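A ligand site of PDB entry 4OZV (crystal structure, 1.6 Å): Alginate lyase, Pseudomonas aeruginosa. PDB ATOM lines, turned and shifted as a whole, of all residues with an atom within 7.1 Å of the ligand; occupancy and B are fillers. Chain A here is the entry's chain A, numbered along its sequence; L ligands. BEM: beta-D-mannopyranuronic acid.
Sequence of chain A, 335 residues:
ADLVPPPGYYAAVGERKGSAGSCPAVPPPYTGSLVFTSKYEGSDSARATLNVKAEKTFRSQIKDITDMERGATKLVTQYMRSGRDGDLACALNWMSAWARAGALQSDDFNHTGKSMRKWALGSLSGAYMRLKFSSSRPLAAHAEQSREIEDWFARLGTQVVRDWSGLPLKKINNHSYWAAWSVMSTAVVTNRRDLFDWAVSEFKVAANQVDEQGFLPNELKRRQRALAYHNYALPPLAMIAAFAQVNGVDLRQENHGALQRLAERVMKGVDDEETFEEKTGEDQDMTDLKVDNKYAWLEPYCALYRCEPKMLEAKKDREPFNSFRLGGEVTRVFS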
ATOM      1  N   PHE A  36      12.928  -6.892  -3.115  1.00  0.00           N
ATOM      2  CA  PHE A  36      14.212  -7.398  -2.631  1.00  0.00           C
ATOM      3  C   PHE A  36      14.719  -6.616  -1.426  1.00  0.00           C
ATOM      4  O   PHE A  36      14.324  -5.467  -1.207  1.00  0.00           O
ATOM      5  CB  PHE A  36      15.264  -7.322  -3.747  1.00  0.00           C
ATOM      6  CG  PHE A  36      14.919  -8.120  -4.980  1.00  0.00           C
ATOM      7  CD1 PHE A  36      14.450  -9.422  -4.892  1.00  0.00           C
ATOM      8  CD2 PHE A  36      15.103  -7.563  -6.232  1.00  0.00           C
ATOM      9  CE1 PHE A  36      14.157 -10.154  -6.037  1.00  0.00           C
ATOM     10  CE2 PHE A  36      14.815  -8.286  -7.390  1.00  0.00           C
ATOM     11  CZ  PHE A  36      14.336  -9.584  -7.283  1.00  0.00           C
ATOM     12  N   THR A  37      15.609  -7.259  -0.675  1.00  0.00           N
ATOM     13  CA  THR A  37      16.275  -6.628   0.465  1.00  0.00           C
ATOM     14  C   THR A  37      17.371  -5.677   0.008  1.00  0.00           C
ATOM     15  O   THR A  37      18.102  -5.966  -0.930  1.00  0.00           O
ATOM     16  CB  THR A  37      16.877  -7.698   1.399  1.00  0.00           C
ATOM     17  OG1 THR A  37      15.844  -8.554   1.872  1.00  0.00           O
ATOM     18  CG2 THR A  37      17.587  -7.061   2.585  1.00  0.00           C
ATOM     19  N   SER A  38      17.475  -4.527   0.673  1.00  0.00           N
ATOM     20  CA  SER A  38      18.534  -3.566   0.382  1.00  0.00           C
ATOM     21  C   SER A  38      19.799  -3.914   1.143  1.00  0.00           C
ATOM     22  O   SER A  38      19.745  -4.279   2.319  1.00  0.00           O
ATOM     23  CB  SER A  38      18.098  -2.146   0.736  1.00  0.00           C
ATOM     24  OG  SER A  38      19.200  -1.254   0.712  1.00  0.00           O
ATOM     25  N   LYS A  39      20.944  -3.799   0.474  1.00  0.00           N
ATOM     26  CA  LYS A  39      22.205  -4.123   1.124  1.00  0.00           C
ATOM     27  C   LYS A  39      22.544  -3.112   2.213  1.00  0.00           C
ATOM     28  O   LYS A  39      23.435  -3.348   3.030  1.00  0.00           O
ATOM     29  CB  LYS A  39      23.331  -4.206   0.098  1.00  0.00           C
ATOM     30  CG  LYS A  39      23.745  -2.881  -0.519  1.00  0.00           C
ATOM     31  CD  LYS A  39      25.123  -3.003  -1.159  1.00  0.00           C
ATOM     32  CE  LYS A  39      25.515  -1.743  -1.894  1.00  0.00           C
ATOM     33  NZ  LYS A  39      24.868  -1.666  -3.227  1.00  0.00           N
ATOM     34  N   TYR A  40      21.826  -1.988   2.230  1.00  0.00           N
ATOM     35  CA  TYR A  40      22.039  -0.959   3.232  1.00  0.00           C
ATOM     36  C   TYR A  40      20.952  -0.983   4.309  1.00  0.00           C
ATOM     37  O   TYR A  40      20.775  -0.010   5.037  1.00  0.00           O
ATOM     38  CB  TYR A  40      22.086   0.434   2.587  1.00  0.00           C
ATOM     39  CG  TYR A  40      23.295   0.700   1.720  1.00  0.00           C
ATOM     40  CD1 TYR A  40      24.581   0.631   2.239  1.00  0.00           C
ATOM     41  CD2 TYR A  40      23.145   1.035   0.376  1.00  0.00           C
ATOM     42  CE1 TYR A  40      25.685   0.886   1.444  1.00  0.00           C
ATOM     43  CE2 TYR A  40      24.249   1.289  -0.419  1.00  0.00           C
ATOM     44  CZ  TYR A  40      25.505   1.208   0.115  1.00  0.00           C
ATOM     45  OH  TYR A  40      26.614   1.461  -0.671  1.00  0.00           O
ATOM     46  N   GLU A  41      20.226  -2.092   4.386  1.00  0.00           N
ATOM     47  CA  GLU A  41      19.122  -2.223   5.334  1.00  0.00           C
ATOM     48  C   GLU A  41      19.571  -1.928   6.763  1.00  0.00           C
ATOM     49  O   GLU A  41      20.540  -2.518   7.253  1.00  0.00           O
ATOM     50  CB  GLU A  41      18.523  -3.630   5.268  1.00  0.00           C
ATOM     51  CG  GLU A  41      17.259  -3.826   6.075  1.00  0.00           C
ATOM     52  CD  GLU A  41      16.730  -5.243   5.988  1.00  0.00           C
ATOM     53  OE1 GLU A  41      17.219  -6.099   6.747  1.00  0.00           O
ATOM     54  OE2 GLU A  41      15.840  -5.497   5.147  1.00  0.00           O
ATOM     55  N   SER A  43      20.490   1.206   7.796  1.00  0.00           N
ATOM     56  CA  SER A  43      21.286   2.440   7.807  1.00  0.00           C
ATOM     57  C   SER A  43      20.430   3.652   8.158  1.00  0.00           C
ATOM     58  O   SER A  43      19.200   3.593   8.123  1.00  0.00           O
ATOM     59  CB  SER A  43      21.969   2.661   6.454  1.00  0.00           C
ATOM     60  OG  SER A  43      22.731   1.540   6.070  1.00  0.00           O
ATOM     61  N   ARG A  47      22.200   6.205   4.072  1.00  0.00           N
ATOM     62  CA  ARG A  47      22.132   4.909   3.393  1.00  0.00           C
ATOM     63  C   ARG A  47      23.513   4.418   2.962  1.00  0.00           C
ATOM     64  O   ARG A  47      23.705   4.011   1.815  1.00  0.00           O
ATOM     65  CB  ARG A  47      21.194   4.977   2.184  1.00  0.00           C
ATOM     66  CG  ARG A  47      19.760   5.402   2.527  1.00  0.00           C
ATOM     67  CD  ARG A  47      19.086   4.401   3.466  1.00  0.00           C
ATOM     68  NE  ARG A  47      18.957   3.069   2.863  1.00  0.00           N
ATOM     69  CZ  ARG A  47      18.437   2.016   3.477  1.00  0.00           C
ATOM     70  NH1 ARG A  47      18.363   0.846   2.849  1.00  0.00           N
ATOM     71  NH2 ARG A  47      17.981   2.126   4.712  1.00  0.00           N
ATOM     72  N   ALA A  48      24.471   4.484   3.879  1.00  0.00           N
ATOM     73  CA  ALA A  48      25.862   4.197   3.541  1.00  0.00           C
ATOM     74  C   ALA A  48      26.484   3.163   4.470  1.00  0.00           C
ATOM     75  O   ALA A  48      27.682   2.889   4.378  1.00  0.00           O
ATOM     76  CB  ALA A  48      26.675   5.488   3.553  1.00  0.00           C
ATOM     77  N   PHE A  58      20.202 -10.153  -0.338  1.00  0.00           N
ATOM     78  CA  PHE A  58      20.026  -9.446  -1.607  1.00  0.00           C
ATOM     79  C   PHE A  58      20.637 -10.198  -2.786  1.00  0.00           C
ATOM     80  O   PHE A  58      19.918 -10.533  -3.743  1.00  0.00           O
ATOM     81  CB  PHE A  58      20.640  -8.034  -1.501  1.00  0.00           C
ATOM     82  CG  PHE A  58      20.789  -7.319  -2.820  1.00  0.00           C
ATOM     83  CD1 PHE A  58      19.690  -7.021  -3.607  1.00  0.00           C
ATOM     84  CD2 PHE A  58      22.047  -6.918  -3.254  1.00  0.00           C
ATOM     85  CE1 PHE A  58      19.845  -6.341  -4.806  1.00  0.00           C
ATOM     86  CE2 PHE A  58      22.202  -6.238  -4.453  1.00  0.00           C
ATOM     87  CZ  PHE A  58      21.097  -5.948  -5.227  1.00  0.00           C
ATOM     88  N   HIS A 111      11.935  -0.368  -4.163  1.00  0.00           N
ATOM     89  CA  HIS A 111      13.001   0.427  -4.785  1.00  0.00           C
ATOM     90  C   HIS A 111      14.142  -0.450  -5.301  1.00  0.00           C
ATOM     91  O   HIS A 111      14.618  -0.264  -6.408  1.00  0.00           O
ATOM     92  CB  HIS A 111      13.547   1.462  -3.803  1.00  0.00           C
ATOM     93  CG  HIS A 111      14.601   2.344  -4.390  1.00  0.00           C
ATOM     94  ND1 HIS A 111      15.946   2.045  -4.338  1.00  0.00           N
ATOM     95  CD2 HIS A 111      14.514   3.528  -5.054  1.00  0.00           C
ATOM     96  CE1 HIS A 111      16.639   2.994  -4.945  1.00  0.00           C
ATOM     97  NE2 HIS A 111      15.784   3.903  -5.383  1.00  0.00           N
ATOM     98  N   THR A 112      14.545  -1.427  -4.489  1.00  0.00           N
ATOM     99  CA  THR A 112      15.637  -2.324  -4.862  1.00  0.00           C
ATOM    100  C   THR A 112      15.286  -3.162  -6.087  1.00  0.00           C
ATOM    101  O   THR A 112      16.128  -3.392  -6.973  1.00  0.00           O
ATOM    102  CB  THR A 112      16.005  -3.244  -3.677  1.00  0.00           C
ATOM    103  OG1 THR A 112      16.321  -2.435  -2.531  1.00  0.00           O
ATOM    104  CG2 THR A 112      17.196  -4.118  -4.021  1.00  0.00           C
ATOM    105  N   GLY A 113      14.039  -3.634  -6.132  1.00  0.00           N
ATOM    106  CA  GLY A 113      13.577  -4.441  -7.238  1.00  0.00           C
ATOM    107  C   GLY A 113      13.491  -3.697  -8.554  1.00  0.00           C
ATOM    108  O   GLY A 113      13.889  -4.220  -9.597  1.00  0.00           O
ATOM    109  N   SER A 115      15.249  -1.187  -9.258  1.00  0.00           N
ATOM    110  CA  SER A 115      16.652  -0.966  -9.577  1.00  0.00           C
ATOM    111  C   SER A 115      17.224  -2.160 -10.334  1.00  0.00           C
ATOM    112  O   SER A 115      18.026  -1.970 -11.245  1.00  0.00           O
ATOM    113  CB  SER A 115      17.477  -0.708  -8.309  1.00  0.00           C
ATOM    114  OG  SER A 115      17.115   0.541  -7.725  1.00  0.00           O
ATOM    115  N   MET A 116      16.815  -3.369  -9.969  1.00  0.00           N
ATOM    116  CA  MET A 116      17.295  -4.568 -10.660  1.00  0.00           C
ATOM    117  C   MET A 116      16.744  -4.623 -12.088  1.00  0.00           C
ATOM    118  O   MET A 116      17.444  -5.050 -13.011  1.00  0.00           O
ATOM    119  CB  MET A 116      16.909  -5.841  -9.909  1.00  0.00           C
ATOM    120  CG  MET A 116      17.667  -6.054  -8.609  1.00  0.00           C
ATOM    121  SD  MET A 116      19.450  -6.011  -8.869  1.00  0.00           S
ATOM    122  CE  MET A 116      19.628  -7.321 -10.087  1.00  0.00           C
ATOM    123  N   LYS A 118      16.049  -2.091 -14.102  1.00  0.00           N
ATOM    124  CA  LYS A 118      16.753  -1.193 -15.008  1.00  0.00           C
ATOM    125  C   LYS A 118      18.211  -1.617 -15.201  1.00  0.00           C
ATOM    126  O   LYS A 118      18.755  -1.462 -16.284  1.00  0.00           O
ATOM    127  CB  LYS A 118      16.655   0.270 -14.528  1.00  0.00           C
ATOM    128  CG  LYS A 118      17.196   0.538 -13.136  1.00  0.00           C
ATOM    129  CD  LYS A 118      18.627   1.029 -13.173  1.00  0.00           C
ATOM    130  CE  LYS A 118      18.994   1.757 -11.896  1.00  0.00           C
ATOM    131  NZ  LYS A 118      19.462   0.830 -10.854  1.00  0.00           N
ATOM    132  N   TRP A 119      18.823  -2.200 -14.167  1.00  0.00           N
ATOM    133  CA  TRP A 119      20.209  -2.645 -14.309  1.00  0.00           C
ATOM    134  C   TRP A 119      20.327  -3.762 -15.347  1.00  0.00           C
ATOM    135  O   TRP A 119      21.196  -3.719 -16.221  1.00  0.00           O
ATOM    136  CB  TRP A 119      20.784  -3.107 -12.971  1.00  0.00           C
ATOM    137  CG  TRP A 119      21.363  -1.977 -12.132  1.00  0.00           C
ATOM    138  CD1 TRP A 119      21.890  -0.781 -12.593  1.00  0.00           C
ATOM    139  CD2 TRP A 119      21.448  -1.928 -10.700  1.00  0.00           C
ATOM    140  NE1 TRP A 119      22.296  -0.010 -11.519  1.00  0.00           N
ATOM    141  CE2 TRP A 119      22.043  -0.691 -10.356  1.00  0.00           C
ATOM    142  CE3 TRP A 119      21.091  -2.816  -9.680  1.00  0.00           C
ATOM    143  CZ2 TRP A 119      22.285  -0.333  -9.029  1.00  0.00           C
ATOM    144  CZ3 TRP A 119      21.334  -2.448  -8.375  1.00  0.00           C
ATOM    145  CH2 TRP A 119      21.925  -1.219  -8.053  1.00  0.00           C
ATOM    146  N   ASN A 173      18.677  10.413  -8.093  1.00  0.00           N
ATOM    147  CA  ASN A 173      20.100  10.266  -7.858  1.00  0.00           C
ATOM    148  C   ASN A 173      20.700   9.317  -8.891  1.00  0.00           C
ATOM    149  O   ASN A 173      20.130   9.148  -9.976  1.00  0.00           O
ATOM    150  CB  ASN A 173      20.353   9.773  -6.417  1.00  0.00           C
ATOM    151  CG  ASN A 173      19.981   8.316  -6.205  1.00  0.00           C
ATOM    152  OD1 ASN A 173      19.335   7.686  -7.050  1.00  0.00           O
ATOM    153  ND2 ASN A 173      20.379   7.763  -5.061  1.00  0.00           N
ATOM    154  N   ASN A 174      21.846   8.708  -8.592  1.00  0.00           N
ATOM    155  CA  ASN A 174      22.493   7.871  -9.584  1.00  0.00           C
ATOM    156  C   ASN A 174      21.568   6.777 -10.141  1.00  0.00           C
ATOM    157  O   ASN A 174      21.734   6.378 -11.294  1.00  0.00           O
ATOM    158  CB  ASN A 174      23.763   7.242  -9.009  1.00  0.00           C
ATOM    159  CG  ASN A 174      23.485   6.297  -7.882  1.00  0.00           C
ATOM    160  OD1 ASN A 174      23.232   5.113  -8.100  1.00  0.00           O
ATOM    161  ND2 ASN A 174      23.533   6.809  -6.657  1.00  0.00           N
ATOM    162  N   HIS A 175      20.573   6.334  -9.376  1.00  0.00           N
ATOM    163  CA  HIS A 175      19.663   5.319  -9.890  1.00  0.00           C
ATOM    164  C   HIS A 175      18.883   5.809 -11.101  1.00  0.00           C
ATOM    165  O   HIS A 175      18.696   5.075 -12.062  1.00  0.00           O
ATOM    166  CB  HIS A 175      18.689   4.844  -8.813  1.00  0.00           C
ATOM    167  CG  HIS A 175      19.280   3.830  -7.885  1.00  0.00           C
ATOM    168  ND1 HIS A 175      19.506   2.525  -8.257  1.00  0.00           N
ATOM    169  CD2 HIS A 175      19.708   3.935  -6.611  1.00  0.00           C
ATOM    170  CE1 HIS A 175      20.039   1.861  -7.252  1.00  0.00           C
ATOM    171  NE2 HIS A 175      20.168   2.696  -6.237  1.00  0.00           N
ATOM    172  N   ARG A 222      25.749  10.689   0.821  1.00  0.00           N
ATOM    173  CA  ARG A 222      26.212   9.335   1.100  1.00  0.00           C
ATOM    174  C   ARG A 222      27.512   9.352   1.922  1.00  0.00           C
ATOM    175  O   ARG A 222      28.154   8.322   2.086  1.00  0.00           O
ATOM    176  CB  ARG A 222      26.417   8.550  -0.198  1.00  0.00           C
ATOM    177  CG  ARG A 222      25.207   8.560  -1.140  1.00  0.00           C
ATOM    178  CD  ARG A 222      23.910   8.104  -0.457  1.00  0.00           C
ATOM    179  NE  ARG A 222      23.845   6.660  -0.270  1.00  0.00           N
ATOM    180  CZ  ARG A 222      23.481   5.800  -1.221  1.00  0.00           C
ATOM    181  NH1 ARG A 222      23.440   4.493  -0.964  1.00  0.00           N
ATOM    182  NH2 ARG A 222      23.171   6.244  -2.425  1.00  0.00           N
ATOM    183  N   TYR A 229      30.153   7.551  -5.130  1.00  0.00           N
ATOM    184  CA  TYR A 229      28.864   7.664  -5.804  1.00  0.00           C
ATOM    185  C   TYR A 229      28.863   8.765  -6.866  1.00  0.00           C
ATOM    186  O   TYR A 229      28.122   8.676  -7.834  1.00  0.00           O
ATOM    187  CB  TYR A 229      27.735   7.863  -4.778  1.00  0.00           C
ATOM    188  CG  TYR A 229      27.175   6.542  -4.274  1.00  0.00           C
ATOM    189  CD1 TYR A 229      26.458   5.703  -5.117  1.00  0.00           C
ATOM    190  CD2 TYR A 229      27.382   6.127  -2.956  1.00  0.00           C
ATOM    191  CE1 TYR A 229      25.952   4.491  -4.672  1.00  0.00           C
ATOM    192  CE2 TYR A 229      26.880   4.904  -2.503  1.00  0.00           C
ATOM    193  CZ  TYR A 229      26.169   4.095  -3.368  1.00  0.00           C
ATOM    194  OH  TYR A 229      25.670   2.892  -2.936  1.00  0.00           O
ATOM    195  N   TYR A 232      30.260   6.934  -9.696  1.00  0.00           N
ATOM    196  CA  TYR A 232      29.242   6.003 -10.166  1.00  0.00           C
ATOM    197  C   TYR A 232      28.213   6.699 -11.060  1.00  0.00           C
ATOM    198  O   TYR A 232      27.603   6.069 -11.926  1.00  0.00           O
ATOM    199  CB  TYR A 232      28.556   5.336  -8.979  1.00  0.00           C
ATOM    200  CG  TYR A 232      27.636   4.176  -9.327  1.00  0.00           C
ATOM    201  CD1 TYR A 232      28.099   3.108 -10.101  1.00  0.00           C
ATOM    202  CD2 TYR A 232      26.323   4.135  -8.873  1.00  0.00           C
ATOM    203  CE1 TYR A 232      27.267   2.057 -10.421  1.00  0.00           C
ATOM    204  CE2 TYR A 232      25.485   3.075  -9.180  1.00  0.00           C
ATOM    205  CZ  TYR A 232      25.965   2.033  -9.959  1.00  0.00           C
ATOM    206  OH  TYR A 232      25.138   0.970 -10.284  1.00  0.00           O
HETATM  207  C1  BEM L   1      22.022   1.689  -3.782  1.00  0.00           C
HETATM  208  C2  BEM L   1      21.729   0.281  -4.302  1.00  0.00           C
HETATM  209  O2  BEM L   1      22.409  -0.676  -3.487  1.00  0.00           O
HETATM  210  C3  BEM L   1      20.225  -0.010  -4.314  1.00  0.00           C
HETATM  211  O3  BEM L   1      19.999  -1.378  -4.654  1.00  0.00           O
HETATM  212  C4  BEM L   1      19.614   0.290  -2.951  1.00  0.00           C
HETATM  213  O4  BEM L   1      18.206   0.044  -2.987  1.00  0.00           O
HETATM  214  C5  BEM L   1      19.924   1.748  -2.596  1.00  0.00           C
HETATM  215  O5  BEM L   1      21.339   1.950  -2.549  1.00  0.00           O
HETATM  216  C6  BEM L   1      19.344   2.144  -1.268  1.00  0.00           C
HETATM  217  O6B BEM L   1      19.881   1.677  -0.251  1.00  0.00           O
HETATM  218  O6A BEM L   1      18.693   3.205  -1.233  1.00  0.00           O
HETATM  219  O1  BEM L   1      23.433   1.848  -3.588  1.00  0.00           O
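Residues that only touch the ligand: Tyr 40 (3.3 Å), Trp 119 (3.9 Å), His 175 (3.2 Å) and Arg 222 (3.7 Å). Hydrophobic or aromatic side chains that line the ligand: Tyr 40, His 111, Trp 119, His 175 and Tyr 229. Within 4 Å of the ligand: Ser 38, Lys 39, Tyr 40, Arg 47, His 111, Thr 112, Trp 119, His 175, Arg 222 and Tyr 229.
OG of Ser 38 is in hydrogen-bond range of NH1 of Arg 47, 3.1 Å away. O of His 111 is in hydrogen-bond range of OG of Ser 115 (2.9 Å). The side-chain hydroxyl (OG) of Ser 38 lies close to the backbone NH (N) of Tyr 40 (3.1 Å). O of Tyr 40 is in hydrogen-bond range of OG of Ser 43 (2.7 Å). The backbone carbonyl oxygen (O) of Arg 47 sits at hydrogen-bond distance from the guanidinium group (NH1) of Arg 222, 2.8 Å away. The guanidinium group (NH1) of Arg 47 sits at hydrogen-bond distance from the backbone carbonyl oxygen (O) of Tyr 40, at 3.4 Å. ND1 of His 175 sits at hydrogen-bond distance from OG of Ser 115, at 3.2 Å. A ring nitrogen (ND1) of His 175 sits at hydrogen-bond distance from the side-chain amino group (NZ) of Lys 118 (3.1 Å).
A ring nitrogen (ND1) of His 111 sits at hydrogen-bond distance from an oxygen (O4) of the ligand, 3.3 Å away. The side-chain hydroxyl (OG) of Ser 38 sits at hydrogen-bond distance from an oxygen (O6B) of the ligand. The side-chain amino group (NZ) of Lys 39 lies within hydrogen-bond range of an oxygen (O2) of the ligand, 2.7 Å away. The guanidinium group of Arg 47 is in salt-bridge range of an oxygen (O6B) of the ligand (3.5 Å). An oxygen (O4) of the ligand sits at hydrogen-bond distance from the side-chain hydroxyl of Thr 112 (3.1 Å). An oxygen (O1) of the ligand lies within hydrogen-bond range of the side-chain hydroxyl (OH) of Tyr 229 (2.6 Å).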
